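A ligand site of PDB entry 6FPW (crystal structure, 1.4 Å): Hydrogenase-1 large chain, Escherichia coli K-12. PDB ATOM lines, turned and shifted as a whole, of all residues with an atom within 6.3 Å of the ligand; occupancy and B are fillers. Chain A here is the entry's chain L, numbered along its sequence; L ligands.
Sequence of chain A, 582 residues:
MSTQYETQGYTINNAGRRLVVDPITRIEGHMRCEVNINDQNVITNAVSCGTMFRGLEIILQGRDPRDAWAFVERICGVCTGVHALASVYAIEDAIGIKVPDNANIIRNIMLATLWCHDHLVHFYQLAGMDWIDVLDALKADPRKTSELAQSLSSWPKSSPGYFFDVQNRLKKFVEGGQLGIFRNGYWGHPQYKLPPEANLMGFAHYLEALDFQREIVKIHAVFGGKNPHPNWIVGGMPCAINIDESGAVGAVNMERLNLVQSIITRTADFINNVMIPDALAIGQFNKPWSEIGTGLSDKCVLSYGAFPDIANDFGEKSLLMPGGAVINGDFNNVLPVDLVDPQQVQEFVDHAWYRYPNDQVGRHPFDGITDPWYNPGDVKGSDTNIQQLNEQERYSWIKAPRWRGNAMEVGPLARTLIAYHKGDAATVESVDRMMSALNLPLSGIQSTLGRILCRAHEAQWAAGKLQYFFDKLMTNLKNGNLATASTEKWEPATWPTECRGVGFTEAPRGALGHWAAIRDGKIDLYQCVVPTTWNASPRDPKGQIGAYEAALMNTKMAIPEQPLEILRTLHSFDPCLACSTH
NI1 of the ligand is bound by SG of Cys 576 (2.2 Å). The side-chain sulfur (SG) of Cys 76 is bound to a nickel atom (NI1) of the ligand. The side-chain sulfur (SG) of Cys 79 binds a nickel atom (NI1) of the ligand, 2.3 Å away. An iron atom (FE1) of the ligand is bound by the side-chain sulfur of Cys 579. The backbone NH of Thr 532 sits at hydrogen-bond distance from a nitrogen (N1) of the ligand. The side-chain hydroxyl of Thr 532 sits at hydrogen-bond distance from a nitrogen (N1) of the ligand, 2.8 Å away. The backbone NH of Arg 509 is in hydrogen-bond range of a nitrogen (N2) of the ligand, 3.0 Å away. NH1 of Arg 509 sits at hydrogen-bond distance from N2 of the ligand (3.1 Å). O1 of the ligand sits at hydrogen-bond distance from NE2 of His 83 (3.5 Å).
The side-chain hydroxyl of Thr 532 lies within hydrogen-bond range of the backbone NH of Cys 576 (3.1 Å). The side-chain sulfur (SG) of Cys 576 sits close to the side-chain carboxylate (OE1) of Glu 28, at 3.4 Å. The side-chain sulfur (SG) of Cys 76 lies close to the backbone NH (N) of Val 78, 3.4 Å away. The side-chain sulfur of Cys 579 lies close to a ring nitrogen (NE2) of His 83 (3.3 Å). OD2 of Asp 118 is in salt-bridge range of NH1 of Arg 509, at 2.8 Å. OD1 of Asp 574 lies within salt-bridge range of NH2 of Arg 509, at 2.7 Å. The side-chain hydroxyl (OG1) of Thr 533 sits close to the backbone carbonyl oxygen (O) of Val 530 (3.2 Å).
The backbone nitrogen (N) of Pro 508 sits close to a nitrogen (N2) of the ligand (3.4 Å). Residues that only touch the ligand: Val 82, Ala 507, Leu 512, Val 530 and Pro 531. Hydrophobic or aromatic side chains that line the ligand: Val 82, His 83, Ala 507, Pro 508, Leu 512, Val 530 and Pro 531. Within 4 Å of the ligand: Cys 76, Cys 79, Val 82, His 83, Ala 507, Pro 508, Arg 509, Leu 512, Val 530, Pro 531, Thr 532, Cys 576 and Cys 579.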
ATOM      1  N   GLU A  28      17.496  -3.846  11.986  1.00  0.00           N
ATOM      2  CA  GLU A  28      18.719  -3.098  12.024  1.00  0.00           C
ATOM      3  C   GLU A  28      19.642  -3.715  13.089  1.00  0.00           C
ATOM      4  O   GLU A  28      19.232  -3.958  14.242  1.00  0.00           O
ATOM      5  CB  GLU A  28      18.442  -1.626  12.324  1.00  0.00           C
ATOM      6  CG  GLU A  28      19.690  -0.751  12.302  1.00  0.00           C
ATOM      7  CD  GLU A  28      20.487  -0.851  13.592  1.00  0.00           C
ATOM      8  OE1 GLU A  28      19.890  -1.180  14.634  1.00  0.00           O
ATOM      9  OE2 GLU A  28      21.710  -0.582  13.553  1.00  0.00           O
ATOM     10  N   ILE A  75      23.193   7.086  17.144  1.00  0.00           N
ATOM     11  CA  ILE A  75      22.609   5.886  17.718  1.00  0.00           C
ATOM     12  C   ILE A  75      22.067   5.003  16.625  1.00  0.00           C
ATOM     13  O   ILE A  75      22.120   3.775  16.679  1.00  0.00           O
ATOM     14  CB  ILE A  75      21.545   6.212  18.795  1.00  0.00           C
ATOM     15  CG1 ILE A  75      22.294   6.746  20.014  1.00  0.00           C
ATOM     16  CG2 ILE A  75      20.731   4.986  19.100  1.00  0.00           C
ATOM     17  CD1 ILE A  75      21.360   7.347  21.041  1.00  0.00           C
ATOM     18  N   CYS A  76      21.501   5.622  15.536  1.00  0.00           N
ATOM     19  CA  CYS A  76      20.826   4.819  14.547  1.00  0.00           C
ATOM     20  C   CYS A  76      20.685   5.571  13.231  1.00  0.00           C
ATOM     21  O   CYS A  76      20.240   6.711  13.192  1.00  0.00           O
ATOM     22  CB  CYS A  76      19.432   4.430  15.023  1.00  0.00           C
ATOM     23  SG  CYS A  76      18.639   3.236  13.921  1.00  0.00           S
ATOM     24  N   GLY A  77      21.082   4.880  12.149  1.00  0.00           N
ATOM     25  CA  GLY A  77      20.977   5.400  10.798  1.00  0.00           C
ATOM     26  C   GLY A  77      19.715   5.014  10.065  1.00  0.00           C
ATOM     27  O   GLY A  77      19.471   5.545   8.990  1.00  0.00           O
ATOM     28  N   VAL A  78      18.923   4.127  10.667  1.00  0.00           N
ATOM     29  CA  VAL A  78      17.598   3.751  10.160  1.00  0.00           C
ATOM     30  C   VAL A  78      16.582   4.751  10.661  1.00  0.00           C
ATOM     31  O   VAL A  78      15.976   5.453   9.849  1.00  0.00           O
ATOM     32  CB  VAL A  78      17.242   2.291  10.511  1.00  0.00           C
ATOM     33  CG1 VAL A  78      15.876   1.961  10.037  1.00  0.00           C
ATOM     34  CG2 VAL A  78      18.286   1.342   9.954  1.00  0.00           C
ATOM     35  N   CYS A  79      16.487   4.908  11.968  1.00  0.00           N
ATOM     36  CA  CYS A  79      15.668   5.977  12.534  1.00  0.00           C
ATOM     37  C   CYS A  79      16.493   7.272  12.650  1.00  0.00           C
ATOM     38  O   CYS A  79      16.515   7.979  13.660  1.00  0.00           O
ATOM     39  CB  CYS A  79      14.983   5.598  13.829  1.00  0.00           C
ATOM     40  SG  CYS A  79      16.081   5.105  15.192  1.00  0.00           S
ATOM     41  N   THR A  80      17.109   7.646  11.550  1.00  0.00           N
ATOM     42  CA  THR A  80      17.975   8.773  11.528  1.00  0.00           C
ATOM     43  C   THR A  80      17.233  10.085  11.685  1.00  0.00           C
ATOM     44  O   THR A  80      16.330  10.419  10.909  1.00  0.00           O
ATOM     45  CB  THR A  80      18.827   8.780  10.236  1.00  0.00           C
ATOM     46  OG1 THR A  80      19.772   9.868  10.260  1.00  0.00           O
ATOM     47  CG2 THR A  80      18.017   8.897   8.947  1.00  0.00           C
ATOM     48  N   VAL A  82      15.747  11.017  14.603  1.00  0.00           N
ATOM     49  CA  VAL A  82      14.873  11.063  15.732  1.00  0.00           C
ATOM     50  C   VAL A  82      15.631  11.322  17.048  1.00  0.00           C
ATOM     51  O   VAL A  82      15.096  11.965  17.962  1.00  0.00           O
ATOM     52  CB  VAL A  82      13.961   9.809  15.851  1.00  0.00           C
ATOM     53  CG1 VAL A  82      14.691   8.577  16.326  1.00  0.00           C
ATOM     54  CG2 VAL A  82      12.778  10.163  16.720  1.00  0.00           C
ATOM     55  N   HIS A  83      16.842  10.788  17.155  1.00  0.00           N
ATOM     56  CA  HIS A  83      17.624  11.004  18.349  1.00  0.00           C
ATOM     57  C   HIS A  83      18.144  12.422  18.425  1.00  0.00           C
ATOM     58  O   HIS A  83      18.308  12.980  19.500  1.00  0.00           O
ATOM     59  CB  HIS A  83      18.776  10.034  18.438  1.00  0.00           C
ATOM     60  CG  HIS A  83      18.310   8.664  18.719  1.00  0.00           C
ATOM     61  ND1 HIS A  83      17.891   8.293  19.975  1.00  0.00           N
ATOM     62  CD2 HIS A  83      18.225   7.551  17.918  1.00  0.00           C
ATOM     63  CE1 HIS A  83      17.552   7.017  19.927  1.00  0.00           C
ATOM     64  NE2 HIS A  83      17.724   6.546  18.706  1.00  0.00           N
ATOM     65  N   LEU A 114      10.658  11.083   8.290  1.00  0.00           N
ATOM     66  CA  LEU A 114      11.268   9.866   8.805  1.00  0.00           C
ATOM     67  C   LEU A 114      10.233   8.763   8.985  1.00  0.00           C
ATOM     68  O   LEU A 114      10.444   7.630   8.578  1.00  0.00           O
ATOM     69  CB  LEU A 114      12.016  10.147  10.100  1.00  0.00           C
ATOM     70  CG  LEU A 114      12.590   8.860  10.710  1.00  0.00           C
ATOM     71  CD1 LEU A 114      13.695   8.273   9.813  1.00  0.00           C
ATOM     72  CD2 LEU A 114      13.134   9.187  12.089  1.00  0.00           C
ATOM     73  N   ASP A 118      10.874   5.406   6.936  1.00  0.00           N
ATOM     74  CA  ASP A 118      11.214   4.255   7.743  1.00  0.00           C
ATOM     75  C   ASP A 118      10.130   3.197   7.631  1.00  0.00           C
ATOM     76  O   ASP A 118      10.411   1.989   7.414  1.00  0.00           O
ATOM     77  CB  ASP A 118      11.433   4.734   9.183  1.00  0.00           C
ATOM     78  CG  ASP A 118      12.216   3.778  10.017  1.00  0.00           C
ATOM     79  OD1 ASP A 118      12.102   2.535   9.823  1.00  0.00           O
ATOM     80  OD2 ASP A 118      12.916   4.296  10.967  1.00  0.00           O
ATOM     81  N   ALA A 507       9.333   7.912  18.008  1.00  0.00           N
ATOM     82  CA  ALA A 507      10.060   7.420  16.892  1.00  0.00           C
ATOM     83  C   ALA A 507       9.219   6.453  16.092  1.00  0.00           C
ATOM     84  O   ALA A 507       8.207   5.956  16.558  1.00  0.00           O
ATOM     85  CB  ALA A 507      11.323   6.765  17.399  1.00  0.00           C
ATOM     86  N   PRO A 508       9.656   6.097  14.893  1.00  0.00           N
ATOM     87  CA  PRO A 508       8.892   5.079  14.132  1.00  0.00           C
ATOM     88  C   PRO A 508       8.560   3.814  14.941  1.00  0.00           C
ATOM     89  O   PRO A 508       7.506   3.247  14.756  1.00  0.00           O
ATOM     90  CB  PRO A 508       9.811   4.781  12.944  1.00  0.00           C
ATOM     91  CG  PRO A 508      10.517   6.134  12.707  1.00  0.00           C
ATOM     92  CD  PRO A 508      10.729   6.695  14.089  1.00  0.00           C
ATOM     93  N   ARG A 509       9.462   3.397  15.809  1.00  0.00           N
ATOM     94  CA  ARG A 509       9.308   2.174  16.588  1.00  0.00           C
ATOM     95  C   ARG A 509       8.673   2.334  17.941  1.00  0.00           C
ATOM     96  O   ARG A 509       8.429   1.328  18.604  1.00  0.00           O
ATOM     97  CB  ARG A 509      10.674   1.433  16.668  1.00  0.00           C
ATOM     98  CG  ARG A 509      11.119   0.970  15.289  1.00  0.00           C
ATOM     99  CD  ARG A 509      12.593   0.660  15.202  1.00  0.00           C
ATOM    100  NE  ARG A 509      12.912   0.266  13.826  1.00  0.00           N
ATOM    101  CZ  ARG A 509      13.057   1.105  12.827  1.00  0.00           C
ATOM    102  NH1 ARG A 509      13.124   2.396  13.022  1.00  0.00           N
ATOM    103  NH2 ARG A 509      13.201   0.641  11.603  1.00  0.00           N
ATOM    104  N   GLY A 510       8.464   3.571  18.396  1.00  0.00           N
ATOM    105  CA  GLY A 510       7.774   3.817  19.667  1.00  0.00           C
ATOM    106  C   GLY A 510       8.342   4.948  20.491  1.00  0.00           C
ATOM    107  O   GLY A 510       9.062   5.804  20.012  1.00  0.00           O
ATOM    108  N   ALA A 511       8.051   4.891  21.789  1.00  0.00           N
ATOM    109  CA  ALA A 511       8.347   5.963  22.717  1.00  0.00           C
ATOM    110  C   ALA A 511       9.846   6.114  22.972  1.00  0.00           C
ATOM    111  O   ALA A 511      10.481   5.180  23.425  1.00  0.00           O
ATOM    112  CB  ALA A 511       7.627   5.657  24.038  1.00  0.00           C
ATOM    113  N   LEU A 512      10.345   7.309  22.761  1.00  0.00           N
ATOM    114  CA  LEU A 512      11.774   7.648  22.902  1.00  0.00           C
ATOM    115  C   LEU A 512      11.959   8.757  23.917  1.00  0.00           C
ATOM    116  O   LEU A 512      11.286   9.800  23.814  1.00  0.00           O
ATOM    117  CB  LEU A 512      12.318   8.160  21.543  1.00  0.00           C
ATOM    118  CG  LEU A 512      13.762   8.676  21.563  1.00  0.00           C
ATOM    119  CD1 LEU A 512      14.750   7.640  22.002  1.00  0.00           C
ATOM    120  CD2 LEU A 512      14.107   9.236  20.207  1.00  0.00           C
ATOM    121  N   VAL A 530      15.053   3.822  24.675  1.00  0.00           N
ATOM    122  CA  VAL A 530      14.697   3.895  23.250  1.00  0.00           C
ATOM    123  C   VAL A 530      13.598   2.836  22.953  1.00  0.00           C
ATOM    124  O   VAL A 530      13.442   1.888  23.751  1.00  0.00           O
ATOM    125  CB  VAL A 530      15.996   3.698  22.475  1.00  0.00           C
ATOM    126  CG1 VAL A 530      15.825   3.859  21.011  1.00  0.00           C
ATOM    127  CG2 VAL A 530      17.069   4.640  22.965  1.00  0.00           C
ATOM    128  N   PRO A 531      12.781   3.003  21.903  1.00  0.00           N
ATOM    129  CA  PRO A 531      11.653   2.102  21.773  1.00  0.00           C
ATOM    130  C   PRO A 531      11.992   0.609  21.789  1.00  0.00           C
ATOM    131  O   PRO A 531      11.339  -0.164  22.468  1.00  0.00           O
ATOM    132  CB  PRO A 531      10.939   2.523  20.479  1.00  0.00           C
ATOM    133  CG  PRO A 531      11.666   3.726  20.035  1.00  0.00           C
ATOM    134  CD  PRO A 531      12.623   4.152  21.029  1.00  0.00           C
ATOM    135  N   THR A 532      13.019   0.199  21.055  1.00  0.00           N
ATOM    136  CA  THR A 532      13.350  -1.225  21.008  1.00  0.00           C
ATOM    137  C   THR A 532      13.933  -1.646  22.371  1.00  0.00           C
ATOM    138  O   THR A 532      13.917  -2.832  22.682  1.00  0.00           O
ATOM    139  CB  THR A 532      14.245  -1.535  19.806  1.00  0.00           C
ATOM    140  OG1 THR A 532      13.549  -1.199  18.588  1.00  0.00           O
ATOM    141  CG2 THR A 532      14.608  -3.002  19.752  1.00  0.00           C
ATOM    142  N   THR A 533      14.462  -0.696  23.166  1.00  0.00           N
ATOM    143  CA  THR A 533      14.854  -1.062  24.534  1.00  0.00           C
ATOM    144  C   THR A 533      13.634  -1.609  25.275  1.00  0.00           C
ATOM    145  O   THR A 533      13.732  -2.622  25.993  1.00  0.00           O
ATOM    146  CB  THR A 533      15.430   0.123  25.317  1.00  0.00           C
ATOM    147  OG1 THR A 533      16.348   0.901  24.515  1.00  0.00           O
ATOM    148  CG2 THR A 533      16.130  -0.337  26.625  1.00  0.00           C
ATOM    149  N   ASP A 574       9.426  -4.291  14.097  1.00  0.00           N
ATOM    150  CA  ASP A 574      10.480  -3.468  13.485  1.00  0.00           C
ATOM    151  C   ASP A 574      11.691  -3.264  14.448  1.00  0.00           C
ATOM    152  O   ASP A 574      12.011  -2.147  14.839  1.00  0.00           O
ATOM    153  CB  ASP A 574       9.806  -2.175  13.059  1.00  0.00           C
ATOM    154  CG  ASP A 574      10.636  -1.289  12.252  1.00  0.00           C
ATOM    155  OD1 ASP A 574      11.739  -1.667  11.780  1.00  0.00           O
ATOM    156  OD2 ASP A 574      10.126  -0.106  12.097  1.00  0.00           O
ATOM    157  N   PRO A 575      12.373  -4.359  14.823  1.00  0.00           N
ATOM    158  CA  PRO A 575      13.477  -4.224  15.811  1.00  0.00           C
ATOM    159  C   PRO A 575      14.599  -3.323  15.302  1.00  0.00           C
ATOM    160  O   PRO A 575      15.049  -3.483  14.144  1.00  0.00           O
ATOM    161  CB  PRO A 575      13.976  -5.682  15.997  1.00  0.00           C
ATOM    162  CG  PRO A 575      12.818  -6.505  15.554  1.00  0.00           C
ATOM    163  CD  PRO A 575      12.184  -5.757  14.412  1.00  0.00           C
ATOM    164  N   CYS A 576      15.078  -2.446  16.158  1.00  0.00           N
ATOM    165  CA  CYS A 576      16.263  -1.621  15.874  1.00  0.00           C
ATOM    166  C   CYS A 576      17.236  -1.795  17.021  1.00  0.00           C
ATOM    167  O   CYS A 576      17.076  -1.225  18.099  1.00  0.00           O
ATOM    168  CB  CYS A 576      15.844  -0.168  15.731  1.00  0.00           C
ATOM    169  SG  CYS A 576      17.209   0.839  15.102  1.00  0.00           S
ATOM    170  N   LEU A 577      18.192  -2.665  16.792  1.00  0.00           N
ATOM    171  CA  LEU A 577      19.024  -3.077  17.884  1.00  0.00           C
ATOM    172  C   LEU A 577      20.113  -2.093  18.291  1.00  0.00           C
ATOM    173  O   LEU A 577      20.480  -2.013  19.477  1.00  0.00           O
ATOM    174  CB  LEU A 577      19.632  -4.443  17.614  1.00  0.00           C
ATOM    175  CG  LEU A 577      18.668  -5.622  17.879  1.00  0.00           C
ATOM    176  CD1 LEU A 577      18.609  -5.858  19.374  1.00  0.00           C
ATOM    177  CD2 LEU A 577      17.281  -5.455  17.263  1.00  0.00           C
ATOM    178  N   ALA A 578      20.607  -1.333  17.328  1.00  0.00           N
ATOM    179  CA  ALA A 578      21.525  -0.240  17.651  1.00  0.00           C
ATOM    180  C   ALA A 578      20.804   0.804  18.560  1.00  0.00           C
ATOM    181  O   ALA A 578      21.390   1.322  19.517  1.00  0.00           O
ATOM    182  CB  ALA A 578      22.086   0.426  16.437  1.00  0.00           C
ATOM    183  N   CYS A 579      19.535   1.082  18.209  1.00  0.00           N
ATOM    184  CA  CYS A 579      18.720   1.922  19.074  1.00  0.00           C
ATOM    185  C   CYS A 579      18.617   1.336  20.491  1.00  0.00           C
ATOM    186  O   CYS A 579      18.713   2.060  21.462  1.00  0.00           O
ATOM    187  CB  CYS A 579      17.333   2.097  18.486  1.00  0.00           C
ATOM    188  SG  CYS A 579      17.185   3.544  17.466  1.00  0.00           S
ATOM    189  N   SER A 580      18.340   0.044  20.541  1.00  0.00           N
ATOM    190  CA  SER A 580      18.011  -0.578  21.812  1.00  0.00           C
ATOM    191  C   SER A 580      19.122  -0.494  22.816  1.00  0.00           C
ATOM    192  O   SER A 580      18.868  -0.437  24.045  1.00  0.00           O
ATOM    193  CB  SER A 580      17.525  -2.004  21.621  1.00  0.00           C
ATOM    194  OG  SER A 580      18.623  -2.874  21.379  1.00  0.00           O
HETATM  195 FE1  LIG L   1      15.035   3.871  16.779  1.00  0.00          FE
HETATM  196 NI1  LIG L   1      16.745   2.950  15.112  1.00  0.00          NI
HETATM  197  C1  LIG L   1      14.381   2.464  17.828  1.00  0.00           C
HETATM  198  N1  LIG L   1      14.001   1.571  18.462  1.00  0.00           N
HETATM  199  C2  LIG L   1      13.352   4.101  16.004  1.00  0.00           C
HETATM  200  N2  LIG L   1      12.320   4.137  15.499  1.00  0.00           N
HETATM  201  C3  LIG L   1      14.623   5.125  17.908  1.00  0.00           C
HETATM  202  O1  LIG L   1      14.315   5.936  18.682  1.00  0.00           O
